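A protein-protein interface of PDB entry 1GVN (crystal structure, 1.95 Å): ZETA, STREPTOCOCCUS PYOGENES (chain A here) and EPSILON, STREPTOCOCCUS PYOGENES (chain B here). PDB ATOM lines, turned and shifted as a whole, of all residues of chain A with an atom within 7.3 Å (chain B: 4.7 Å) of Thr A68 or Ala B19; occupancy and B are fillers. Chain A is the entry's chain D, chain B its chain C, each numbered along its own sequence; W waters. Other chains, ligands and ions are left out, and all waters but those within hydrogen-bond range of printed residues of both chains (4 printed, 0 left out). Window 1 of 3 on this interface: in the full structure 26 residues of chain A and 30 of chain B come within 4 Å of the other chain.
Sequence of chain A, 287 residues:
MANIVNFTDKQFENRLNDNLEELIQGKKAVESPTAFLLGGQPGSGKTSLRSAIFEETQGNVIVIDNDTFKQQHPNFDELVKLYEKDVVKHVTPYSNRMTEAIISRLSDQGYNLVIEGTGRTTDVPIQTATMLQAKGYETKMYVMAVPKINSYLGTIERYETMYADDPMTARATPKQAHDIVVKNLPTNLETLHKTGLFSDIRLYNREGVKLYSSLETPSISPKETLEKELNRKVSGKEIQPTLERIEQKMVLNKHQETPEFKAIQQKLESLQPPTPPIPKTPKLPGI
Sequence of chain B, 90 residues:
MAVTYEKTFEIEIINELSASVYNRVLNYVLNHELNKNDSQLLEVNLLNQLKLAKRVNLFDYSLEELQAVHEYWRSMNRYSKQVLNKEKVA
The side-chain hydroxyl of Ser B20 lies within hydrogen-bond range of the side-chain amide oxygen of Gln A71 (2.8 Å). ND2 of Asn B23 sits at hydrogen-bond distance from O of Thr A68 (2.8 Å). OD1 of Asn B23 sits close to OE1 of Gln A72 (3.0 Å).
The side-chain hydroxyl of Ser B18 sits at hydrogen-bond distance from the backbone carbonyl oxygen of Asn B15, at 3.3 Å. The backbone carbonyl oxygen (O) of Ala B19 is in hydrogen-bond range of the side-chain amide nitrogen (ND2) of Asn B23, at 3.0 Å. The side-chain amide oxygen (OD1) of Asn A19 lies within hydrogen-bond range of the side-chain amide nitrogen (NE2) of Gln A72, at 2.8 Å. The guanidinium group of Arg A50 lies within salt-bridge range of the side-chain carboxylate of Asp A65. O of Asp A65 is in hydrogen-bond range of OG1 of Thr A68, 2.9 Å away. The side-chain amide nitrogen of Gln A72 is in hydrogen-bond range of the side-chain hydroxyl of Tyr A94, 2.8 Å away.
Among the printed residues, pairs that only touch across the chains: Arg A50 with Asn B15 (3.5 Å), Thr A68 with Ala B19 (3.996 Å) and Gln A71 with Asn B23 (3.8 Å).
Of the printed residues of chain B, Thr A68 touches Ala B19 (3.996 Å) and Asn B23 (2.8 Å). Printed residues of chain A within 4 Å of Ala B19: Thr A68. No residue of chain A comes within 4 Å of Ser B18. Of the printed residues of chain A, Asn B15 touches Arg A50. Of the printed residues of chain A, Ser B20 touches Gln A71 (2.8 Å). Printed residues of chain B within 4 Å of Gln A72: Asn B23 (3.0 Å). Printed residues of chain B within 4 Å of Gln A71: Ser B20 and Asn B23. The nearest printed residue of chain B that does not touch Thr A68 is Asn B15 (4.7 Å). The nearest printed residue of chain A that does not touch Ala B19 is Gln A71 (5.2 Å).
Of the 17 printed residues of chain A, 4 touch a printed residue of chain B. Among the printed residues, 6 pairs touch across the chains. Among the printed residues, no Asp or Glu carboxylate lies within 4 Å of a Lys or Arg side-chain nitrogen of the other chain.
Water W1 bridges the backbone carbonyl oxygen of Glu B16 (2.6 Å) and the side-chain amide nitrogen of Gln A71 (3.4 Å). Water W4 bridges NE2 of Gln A71 (2.7 Å) and ND2 of Asn B23 (2.9 Å). Water W3 lies within hydrogen-bond range of OD1 of Asn B15 (2.8 Å) and NH1 of Arg A50 (3.3 Å). Water W2 bridges O of Ser B20 (2.8 Å) and OE1 of Gln A71 (2.9 Å).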
ATOM      1  N   ASN A  19     -16.889   8.210  19.881  1.00  0.00           N
ATOM      2  CA  ASN A  19     -17.365   9.161  20.884  1.00  0.00           C
ATOM      3  C   ASN A  19     -16.225   9.512  21.845  1.00  0.00           C
ATOM      4  O   ASN A  19     -15.973  10.682  22.133  1.00  0.00           O
ATOM      5  CB  ASN A  19     -18.530   8.549  21.683  1.00  0.00           C
ATOM      6  CG  ASN A  19     -19.831   8.490  20.887  1.00  0.00           C
ATOM      7  OD1 ASN A  19     -20.738   7.717  21.214  1.00  0.00           O
ATOM      8  ND2 ASN A  19     -19.933   9.314  19.852  1.00  0.00           N
ATOM      9  N   LEU A  23     -14.424  13.122  22.460  1.00  0.00           N
ATOM     10  CA  LEU A  23     -14.499  13.758  23.771  1.00  0.00           C
ATOM     11  C   LEU A  23     -13.186  14.037  24.494  1.00  0.00           C
ATOM     12  O   LEU A  23     -13.064  15.058  25.172  1.00  0.00           O
ATOM     13  CB  LEU A  23     -15.414  12.938  24.681  1.00  0.00           C
ATOM     14  CG  LEU A  23     -16.866  12.910  24.200  1.00  0.00           C
ATOM     15  CD1 LEU A  23     -17.631  11.805  24.918  1.00  0.00           C
ATOM     16  CD2 LEU A  23     -17.504  14.281  24.450  1.00  0.00           C
ATOM     17  N   ARG A  50     -21.950  25.446  31.580  1.00  0.00           N
ATOM     18  CA  ARG A  50     -20.808  24.839  30.914  1.00  0.00           C
ATOM     19  C   ARG A  50     -19.685  25.863  30.801  1.00  0.00           C
ATOM     20  O   ARG A  50     -18.516  25.530  30.973  1.00  0.00           O
ATOM     21  CB  ARG A  50     -21.177  24.360  29.516  1.00  0.00           C
ATOM     22  CG  ARG A  50     -22.240  23.292  29.462  1.00  0.00           C
ATOM     23  CD  ARG A  50     -22.335  22.761  28.042  1.00  0.00           C
ATOM     24  NE  ARG A  50     -23.475  21.865  27.867  1.00  0.00           N
ATOM     25  CZ  ARG A  50     -23.630  21.053  26.826  1.00  0.00           C
ATOM     26  NH1 ARG A  50     -22.712  21.021  25.861  1.00  0.00           N
ATOM     27  NH2 ARG A  50     -24.697  20.271  26.753  1.00  0.00           N
ATOM     28  N   VAL A  63     -17.663  17.252  28.540  1.00  0.00           N
ATOM     29  CA  VAL A  63     -19.098  17.375  28.750  1.00  0.00           C
ATOM     30  C   VAL A  63     -19.821  16.165  28.184  1.00  0.00           C
ATOM     31  O   VAL A  63     -19.668  15.836  27.008  1.00  0.00           O
ATOM     32  CB  VAL A  63     -19.662  18.643  28.069  1.00  0.00           C
ATOM     33  CG1 VAL A  63     -21.155  18.777  28.374  1.00  0.00           C
ATOM     34  CG2 VAL A  63     -18.898  19.878  28.547  1.00  0.00           C
ATOM     35  N   ILE A  64     -20.602  15.504  29.033  1.00  0.00           N
ATOM     36  CA  ILE A  64     -21.370  14.331  28.632  1.00  0.00           C
ATOM     37  C   ILE A  64     -22.845  14.727  28.541  1.00  0.00           C
ATOM     38  O   ILE A  64     -23.498  15.004  29.553  1.00  0.00           O
ATOM     39  CB  ILE A  64     -21.180  13.182  29.643  1.00  0.00           C
ATOM     40  CG1 ILE A  64     -19.691  12.820  29.715  1.00  0.00           C
ATOM     41  CG2 ILE A  64     -22.010  11.980  29.230  1.00  0.00           C
ATOM     42  CD1 ILE A  64     -19.366  11.661  30.630  1.00  0.00           C
ATOM     43  N   ASP A  65     -23.351  14.747  27.311  1.00  0.00           N
ATOM     44  CA  ASP A  65     -24.721  15.156  27.006  1.00  0.00           C
ATOM     45  C   ASP A  65     -25.467  14.013  26.310  1.00  0.00           C
ATOM     46  O   ASP A  65     -25.252  13.755  25.129  1.00  0.00           O
ATOM     47  CB  ASP A  65     -24.657  16.373  26.082  1.00  0.00           C
ATOM     48  CG  ASP A  65     -25.999  17.050  25.892  1.00  0.00           C
ATOM     49  OD1 ASP A  65     -27.047  16.413  26.117  1.00  0.00           O
ATOM     50  OD2 ASP A  65     -25.993  18.231  25.494  1.00  0.00           O
ATOM     51  N   ASN A  66     -26.343  13.335  27.045  1.00  0.00           N
ATOM     52  CA  ASN A  66     -27.107  12.213  26.505  1.00  0.00           C
ATOM     53  C   ASN A  66     -27.720  12.463  25.118  1.00  0.00           C
ATOM     54  O   ASN A  66     -27.598  11.632  24.215  1.00  0.00           O
ATOM     55  CB  ASN A  66     -28.230  11.841  27.471  1.00  0.00           C
ATOM     56  CG  ASN A  66     -29.012  10.627  27.011  1.00  0.00           C
ATOM     57  OD1 ASN A  66     -28.652   9.493  27.311  1.00  0.00           O
ATOM     58  ND2 ASN A  66     -30.082  10.863  26.261  1.00  0.00           N
ATOM     59  N   ASP A  67     -28.376  13.606  24.953  1.00  0.00           N
ATOM     60  CA  ASP A  67     -29.024  13.944  23.688  1.00  0.00           C
ATOM     61  C   ASP A  67     -28.154  13.877  22.434  1.00  0.00           C
ATOM     62  O   ASP A  67     -28.652  13.555  21.356  1.00  0.00           O
ATOM     63  CB  ASP A  67     -29.668  15.334  23.778  1.00  0.00           C
ATOM     64  CG  ASP A  67     -30.901  15.351  24.670  1.00  0.00           C
ATOM     65  OD1 ASP A  67     -31.776  14.477  24.489  1.00  0.00           O
ATOM     66  OD2 ASP A  67     -31.002  16.239  25.545  1.00  0.00           O
ATOM     67  N   THR A  68     -26.863  14.165  22.559  1.00  0.00           N
ATOM     68  CA  THR A  68     -25.985  14.141  21.390  1.00  0.00           C
ATOM     69  C   THR A  68     -25.769  12.760  20.770  1.00  0.00           C
ATOM     70  O   THR A  68     -25.128  12.651  19.724  1.00  0.00           O
ATOM     71  CB  THR A  68     -24.587  14.718  21.709  1.00  0.00           C
ATOM     72  OG1 THR A  68     -23.900  13.839  22.608  1.00  0.00           O
ATOM     73  CG2 THR A  68     -24.702  16.104  22.338  1.00  0.00           C
ATOM     74  N   PHE A  69     -26.300  11.712  21.394  1.00  0.00           N
ATOM     75  CA  PHE A  69     -26.105  10.353  20.877  1.00  0.00           C
ATOM     76  C   PHE A  69     -27.340   9.703  20.264  1.00  0.00           C
ATOM     77  O   PHE A  69     -27.240   8.644  19.641  1.00  0.00           O
ATOM     78  CB  PHE A  69     -25.595   9.431  21.989  1.00  0.00           C
ATOM     79  CG  PHE A  69     -24.429   9.984  22.751  1.00  0.00           C
ATOM     80  CD1 PHE A  69     -23.242  10.300  22.099  1.00  0.00           C
ATOM     81  CD2 PHE A  69     -24.521  10.199  24.124  1.00  0.00           C
ATOM     82  CE1 PHE A  69     -22.162  10.826  22.799  1.00  0.00           C
ATOM     83  CE2 PHE A  69     -23.443  10.726  24.840  1.00  0.00           C
ATOM     84  CZ  PHE A  69     -22.263  11.040  24.177  1.00  0.00           C
ATOM     85  N   LYS A  70     -28.501  10.322  20.434  1.00  0.00           N
ATOM     86  CA  LYS A  70     -29.728   9.734  19.910  1.00  0.00           C
ATOM     87  C   LYS A  70     -29.732   9.393  18.421  1.00  0.00           C
ATOM     88  O   LYS A  70     -30.114   8.285  18.043  1.00  0.00           O
ATOM     89  CB  LYS A  70     -30.922  10.628  20.253  1.00  0.00           C
ATOM     90  CG  LYS A  70     -31.261  10.608  21.746  1.00  0.00           C
ATOM     91  CD  LYS A  70     -32.512  11.414  22.062  1.00  0.00           C
ATOM     92  CE  LYS A  70     -32.827  11.381  23.549  1.00  0.00           C
ATOM     93  NZ  LYS A  70     -34.024  12.209  23.878  1.00  0.00           N
ATOM     94  N   GLN A  71     -29.296  10.321  17.577  1.00  0.00           N
ATOM     95  CA  GLN A  71     -29.294  10.076  16.138  1.00  0.00           C
ATOM     96  C   GLN A  71     -28.115   9.226  15.690  1.00  0.00           C
ATOM     97  O   GLN A  71     -27.872   9.048  14.496  1.00  0.00           O
ATOM     98  CB  GLN A  71     -29.294  11.406  15.397  1.00  0.00           C
ATOM     99  CG  GLN A  71     -30.445  12.290  15.817  1.00  0.00           C
ATOM    100  CD  GLN A  71     -30.315  13.693  15.288  1.00  0.00           C
ATOM    101  OE1 GLN A  71     -30.328  13.914  14.074  1.00  0.00           O
ATOM    102  NE2 GLN A  71     -30.182  14.657  16.195  1.00  0.00           N
ATOM    103  N   GLN A  72     -27.403   8.679  16.666  1.00  0.00           N
ATOM    104  CA  GLN A  72     -26.240   7.852  16.411  1.00  0.00           C
ATOM    105  C   GLN A  72     -26.614   6.366  16.376  1.00  0.00           C
ATOM    106  O   GLN A  72     -25.769   5.504  16.118  1.00  0.00           O
ATOM    107  CB  GLN A  72     -25.216   8.133  17.502  1.00  0.00           C
ATOM    108  CG  GLN A  72     -23.805   7.831  17.146  1.00  0.00           C
ATOM    109  CD  GLN A  72     -22.879   8.278  18.240  1.00  0.00           C
ATOM    110  OE1 GLN A  72     -22.231   9.326  18.144  1.00  0.00           O
ATOM    111  NE2 GLN A  72     -22.831   7.503  19.310  1.00  0.00           N
ATOM    112  N   TYR A  94     -30.710   3.405  23.252  1.00  0.00           N
ATOM    113  CA  TYR A  94     -29.343   3.411  22.750  1.00  0.00           C
ATOM    114  C   TYR A  94     -28.575   4.566  23.384  1.00  0.00           C
ATOM    115  O   TYR A  94     -27.485   4.373  23.921  1.00  0.00           O
ATOM    116  CB  TYR A  94     -29.323   3.588  21.228  1.00  0.00           C
ATOM    117  CG  TYR A  94     -27.956   3.956  20.689  1.00  0.00           C
ATOM    118  CD1 TYR A  94     -26.989   2.980  20.454  1.00  0.00           C
ATOM    119  CD2 TYR A  94     -27.613   5.291  20.458  1.00  0.00           C
ATOM    120  CE1 TYR A  94     -25.707   3.324  20.004  1.00  0.00           C
ATOM    121  CE2 TYR A  94     -26.340   5.642  20.011  1.00  0.00           C
ATOM    122  CZ  TYR A  94     -25.393   4.656  19.788  1.00  0.00           C
ATOM    123  OH  TYR A  94     -24.134   4.999  19.356  1.00  0.00           O
ATOM    124  N   SER A  95     -29.148   5.768  23.324  1.00  0.00           N
ATOM    125  CA  SER A  95     -28.474   6.937  23.881  1.00  0.00           C
ATOM    126  C   SER A  95     -28.180   6.762  25.366  1.00  0.00           C
ATOM    127  O   SER A  95     -27.091   7.105  25.833  1.00  0.00           O
ATOM    128  CB  SER A  95     -29.297   8.216  23.642  1.00  0.00           C
ATOM    129  OG  SER A  95     -30.541   8.191  24.320  1.00  0.00           O
ATOM    130  N   THR A  99     -24.487   6.780  26.890  1.00  0.00           N
ATOM    131  CA  THR A  99     -24.144   7.769  27.907  1.00  0.00           C
ATOM    132  C   THR A  99     -23.532   7.094  29.128  1.00  0.00           C
ATOM    133  O   THR A  99     -22.512   7.537  29.651  1.00  0.00           O
ATOM    134  CB  THR A  99     -25.391   8.567  28.347  1.00  0.00           C
ATOM    135  OG1 THR A  99     -25.889   9.326  27.236  1.00  0.00           O
ATOM    136  CG2 THR A  99     -25.048   9.513  29.500  1.00  0.00           C
ATOM    137  N   ILE A 102     -19.975   5.775  28.336  1.00  0.00           N
ATOM    138  CA  ILE A 102     -18.985   6.847  28.293  1.00  0.00           C
ATOM    139  C   ILE A 102     -18.617   7.349  29.688  1.00  0.00           C
ATOM    140  O   ILE A 102     -17.436   7.516  29.993  1.00  0.00           O
ATOM    141  CB  ILE A 102     -19.487   8.019  27.422  1.00  0.00           C
ATOM    142  CG1 ILE A 102     -19.619   7.542  25.972  1.00  0.00           C
ATOM    143  CG2 ILE A 102     -18.523   9.205  27.515  1.00  0.00           C
ATOM    144  CD1 ILE A 102     -20.234   8.555  25.030  1.00  0.00           C
ATOM    145  N   ILE B  14     -26.005  25.350  18.293  1.00  0.00           N
ATOM    146  CA  ILE B  14     -24.888  24.795  17.535  1.00  0.00           C
ATOM    147  C   ILE B  14     -24.572  23.375  18.011  1.00  0.00           C
ATOM    148  O   ILE B  14     -24.366  22.470  17.202  1.00  0.00           O
ATOM    149  CB  ILE B  14     -23.617  25.653  17.698  1.00  0.00           C
ATOM    150  CG1 ILE B  14     -23.792  26.980  16.957  1.00  0.00           C
ATOM    151  CG2 ILE B  14     -22.395  24.900  17.157  1.00  0.00           C
ATOM    152  CD1 ILE B  14     -22.683  27.974  17.225  1.00  0.00           C
ATOM    153  N   ASN B  15     -24.532  23.187  19.325  1.00  0.00           N
ATOM    154  CA  ASN B  15     -24.230  21.880  19.890  1.00  0.00           C
ATOM    155  C   ASN B  15     -25.241  20.809  19.471  1.00  0.00           C
ATOM    156  O   ASN B  15     -24.859  19.666  19.227  1.00  0.00           O
ATOM    157  CB  ASN B  15     -24.145  21.981  21.416  1.00  0.00           C
ATOM    158  CG  ASN B  15     -22.840  22.613  21.889  1.00  0.00           C
ATOM    159  OD1 ASN B  15     -22.750  23.129  23.008  1.00  0.00           O
ATOM    160  ND2 ASN B  15     -21.818  22.563  21.046  1.00  0.00           N
ATOM    161  N   GLU B  16     -26.519  21.170  19.381  1.00  0.00           N
ATOM    162  CA  GLU B  16     -27.533  20.202  18.965  1.00  0.00           C
ATOM    163  C   GLU B  16     -27.439  19.935  17.460  1.00  0.00           C
ATOM    164  O   GLU B  16     -27.464  18.786  17.023  1.00  0.00           O
ATOM    165  CB  GLU B  16     -28.946  20.695  19.302  1.00  0.00           C
ATOM    166  CG  GLU B  16     -29.248  20.775  20.793  1.00  0.00           C
ATOM    167  CD  GLU B  16     -30.738  20.911  21.086  1.00  0.00           C
ATOM    168  OE1 GLU B  16     -31.495  19.968  20.769  1.00  0.00           O
ATOM    169  OE2 GLU B  16     -31.155  21.956  21.633  1.00  0.00           O
ATOM    170  N   LEU B  17     -27.315  20.995  16.669  1.00  0.00           N
ATOM    171  CA  LEU B  17     -27.235  20.837  15.220  1.00  0.00           C
ATOM    172  C   LEU B  17     -25.992  20.075  14.771  1.00  0.00           C
ATOM    173  O   LEU B  17     -26.085  19.172  13.937  1.00  0.00           O
ATOM    174  CB  LEU B  17     -27.280  22.202  14.526  1.00  0.00           C
ATOM    175  CG  LEU B  17     -27.232  22.183  12.992  1.00  0.00           C
ATOM    176  CD1 LEU B  17     -28.380  21.339  12.442  1.00  0.00           C
ATOM    177  CD2 LEU B  17     -27.329  23.614  12.466  1.00  0.00           C
ATOM    178  N   SER B  18     -24.833  20.427  15.326  1.00  0.00           N
ATOM    179  CA  SER B  18     -23.585  19.767  14.950  1.00  0.00           C
ATOM    180  C   SER B  18     -23.626  18.277  15.272  1.00  0.00           C
ATOM    181  O   SER B  18     -23.093  17.462  14.523  1.00  0.00           O
ATOM    182  CB  SER B  18     -22.391  20.421  15.652  1.00  0.00           C
ATOM    183  OG  SER B  18     -22.469  20.274  17.057  1.00  0.00           O
ATOM    184  N   ALA B  19     -24.260  17.922  16.386  1.00  0.00           N
ATOM    185  CA  ALA B  19     -24.370  16.518  16.776  1.00  0.00           C
ATOM    186  C   ALA B  19     -25.131  15.753  15.697  1.00  0.00           C
ATOM    187  O   ALA B  19     -24.709  14.681  15.261  1.00  0.00           O
ATOM    188  CB  ALA B  19     -25.106  16.397  18.120  1.00  0.00           C
ATOM    189  N   SER B  20     -26.256  16.318  15.272  1.00  0.00           N
ATOM    190  CA  SER B  20     -27.090  15.706  14.252  1.00  0.00           C
ATOM    191  C   SER B  20     -26.329  15.491  12.945  1.00  0.00           C
ATOM    192  O   SER B  20     -26.389  14.414  12.352  1.00  0.00           O
ATOM    193  CB  SER B  20     -28.319  16.584  13.998  1.00  0.00           C
ATOM    194  OG  SER B  20     -29.039  16.131  12.870  1.00  0.00           O
ATOM    195  N   VAL B  21     -25.611  16.517  12.504  1.00  0.00           N
ATOM    196  CA  VAL B  21     -24.843  16.446  11.267  1.00  0.00           C
ATOM    197  C   VAL B  21     -23.698  15.441  11.386  1.00  0.00           C
ATOM    198  O   VAL B  21     -23.519  14.575  10.523  1.00  0.00           O
ATOM    199  CB  VAL B  21     -24.266  17.837  10.896  1.00  0.00           C
ATOM    200  CG1 VAL B  21     -23.475  17.754   9.582  1.00  0.00           C
ATOM    201  CG2 VAL B  21     -25.396  18.843  10.763  1.00  0.00           C
ATOM    202  N   TYR B  22     -22.930  15.551  12.463  1.00  0.00           N
ATOM    203  CA  TYR B  22     -21.806  14.648  12.678  1.00  0.00           C
ATOM    204  C   TYR B  22     -22.265  13.194  12.763  1.00  0.00           C
ATOM    205  O   TYR B  22     -21.683  12.314  12.130  1.00  0.00           O
ATOM    206  CB  TYR B  22     -21.060  15.016  13.959  1.00  0.00           C
ATOM    207  CG  TYR B  22     -19.819  14.188  14.183  1.00  0.00           C
ATOM    208  CD1 TYR B  22     -18.614  14.509  13.552  1.00  0.00           C
ATOM    209  CD2 TYR B  22     -19.854  13.062  15.009  1.00  0.00           C
ATOM    210  CE1 TYR B  22     -17.466  13.725  13.739  1.00  0.00           C
ATOM    211  CE2 TYR B  22     -18.724  12.276  15.201  1.00  0.00           C
ATOM    212  CZ  TYR B  22     -17.534  12.610  14.567  1.00  0.00           C
ATOM    213  OH  TYR B  22     -16.419  11.829  14.772  1.00  0.00           O
ATOM    214  N   ASN B  23     -23.307  12.944  13.552  1.00  0.00           N
ATOM    215  CA  ASN B  23     -23.820  11.585  13.702  1.00  0.00           C
ATOM    216  C   ASN B  23     -24.240  10.979  12.361  1.00  0.00           C
ATOM    217  O   ASN B  23     -23.969   9.805  12.090  1.00  0.00           O
ATOM    218  CB  ASN B  23     -24.996  11.559  14.685  1.00  0.00           C
ATOM    219  CG  ASN B  23     -24.561  11.811  16.120  1.00  0.00           C
ATOM    220  OD1 ASN B  23     -23.437  11.494  16.494  1.00  0.00           O
ATOM    221  ND2 ASN B  23     -25.460  12.366  16.934  1.00  0.00           N
HETATM  222  O   HOH W   1     -28.501  16.750  18.325  1.00  0.00           O
HETATM  223  O   HOH W   2     -28.574  12.605  12.156  1.00  0.00           O
HETATM  224  O   HOH W   3     -24.846  23.400  24.885  1.00  0.00           O
HETATM  225  O   HOH W   4     -28.126  13.458  17.523  1.00  0.00           O
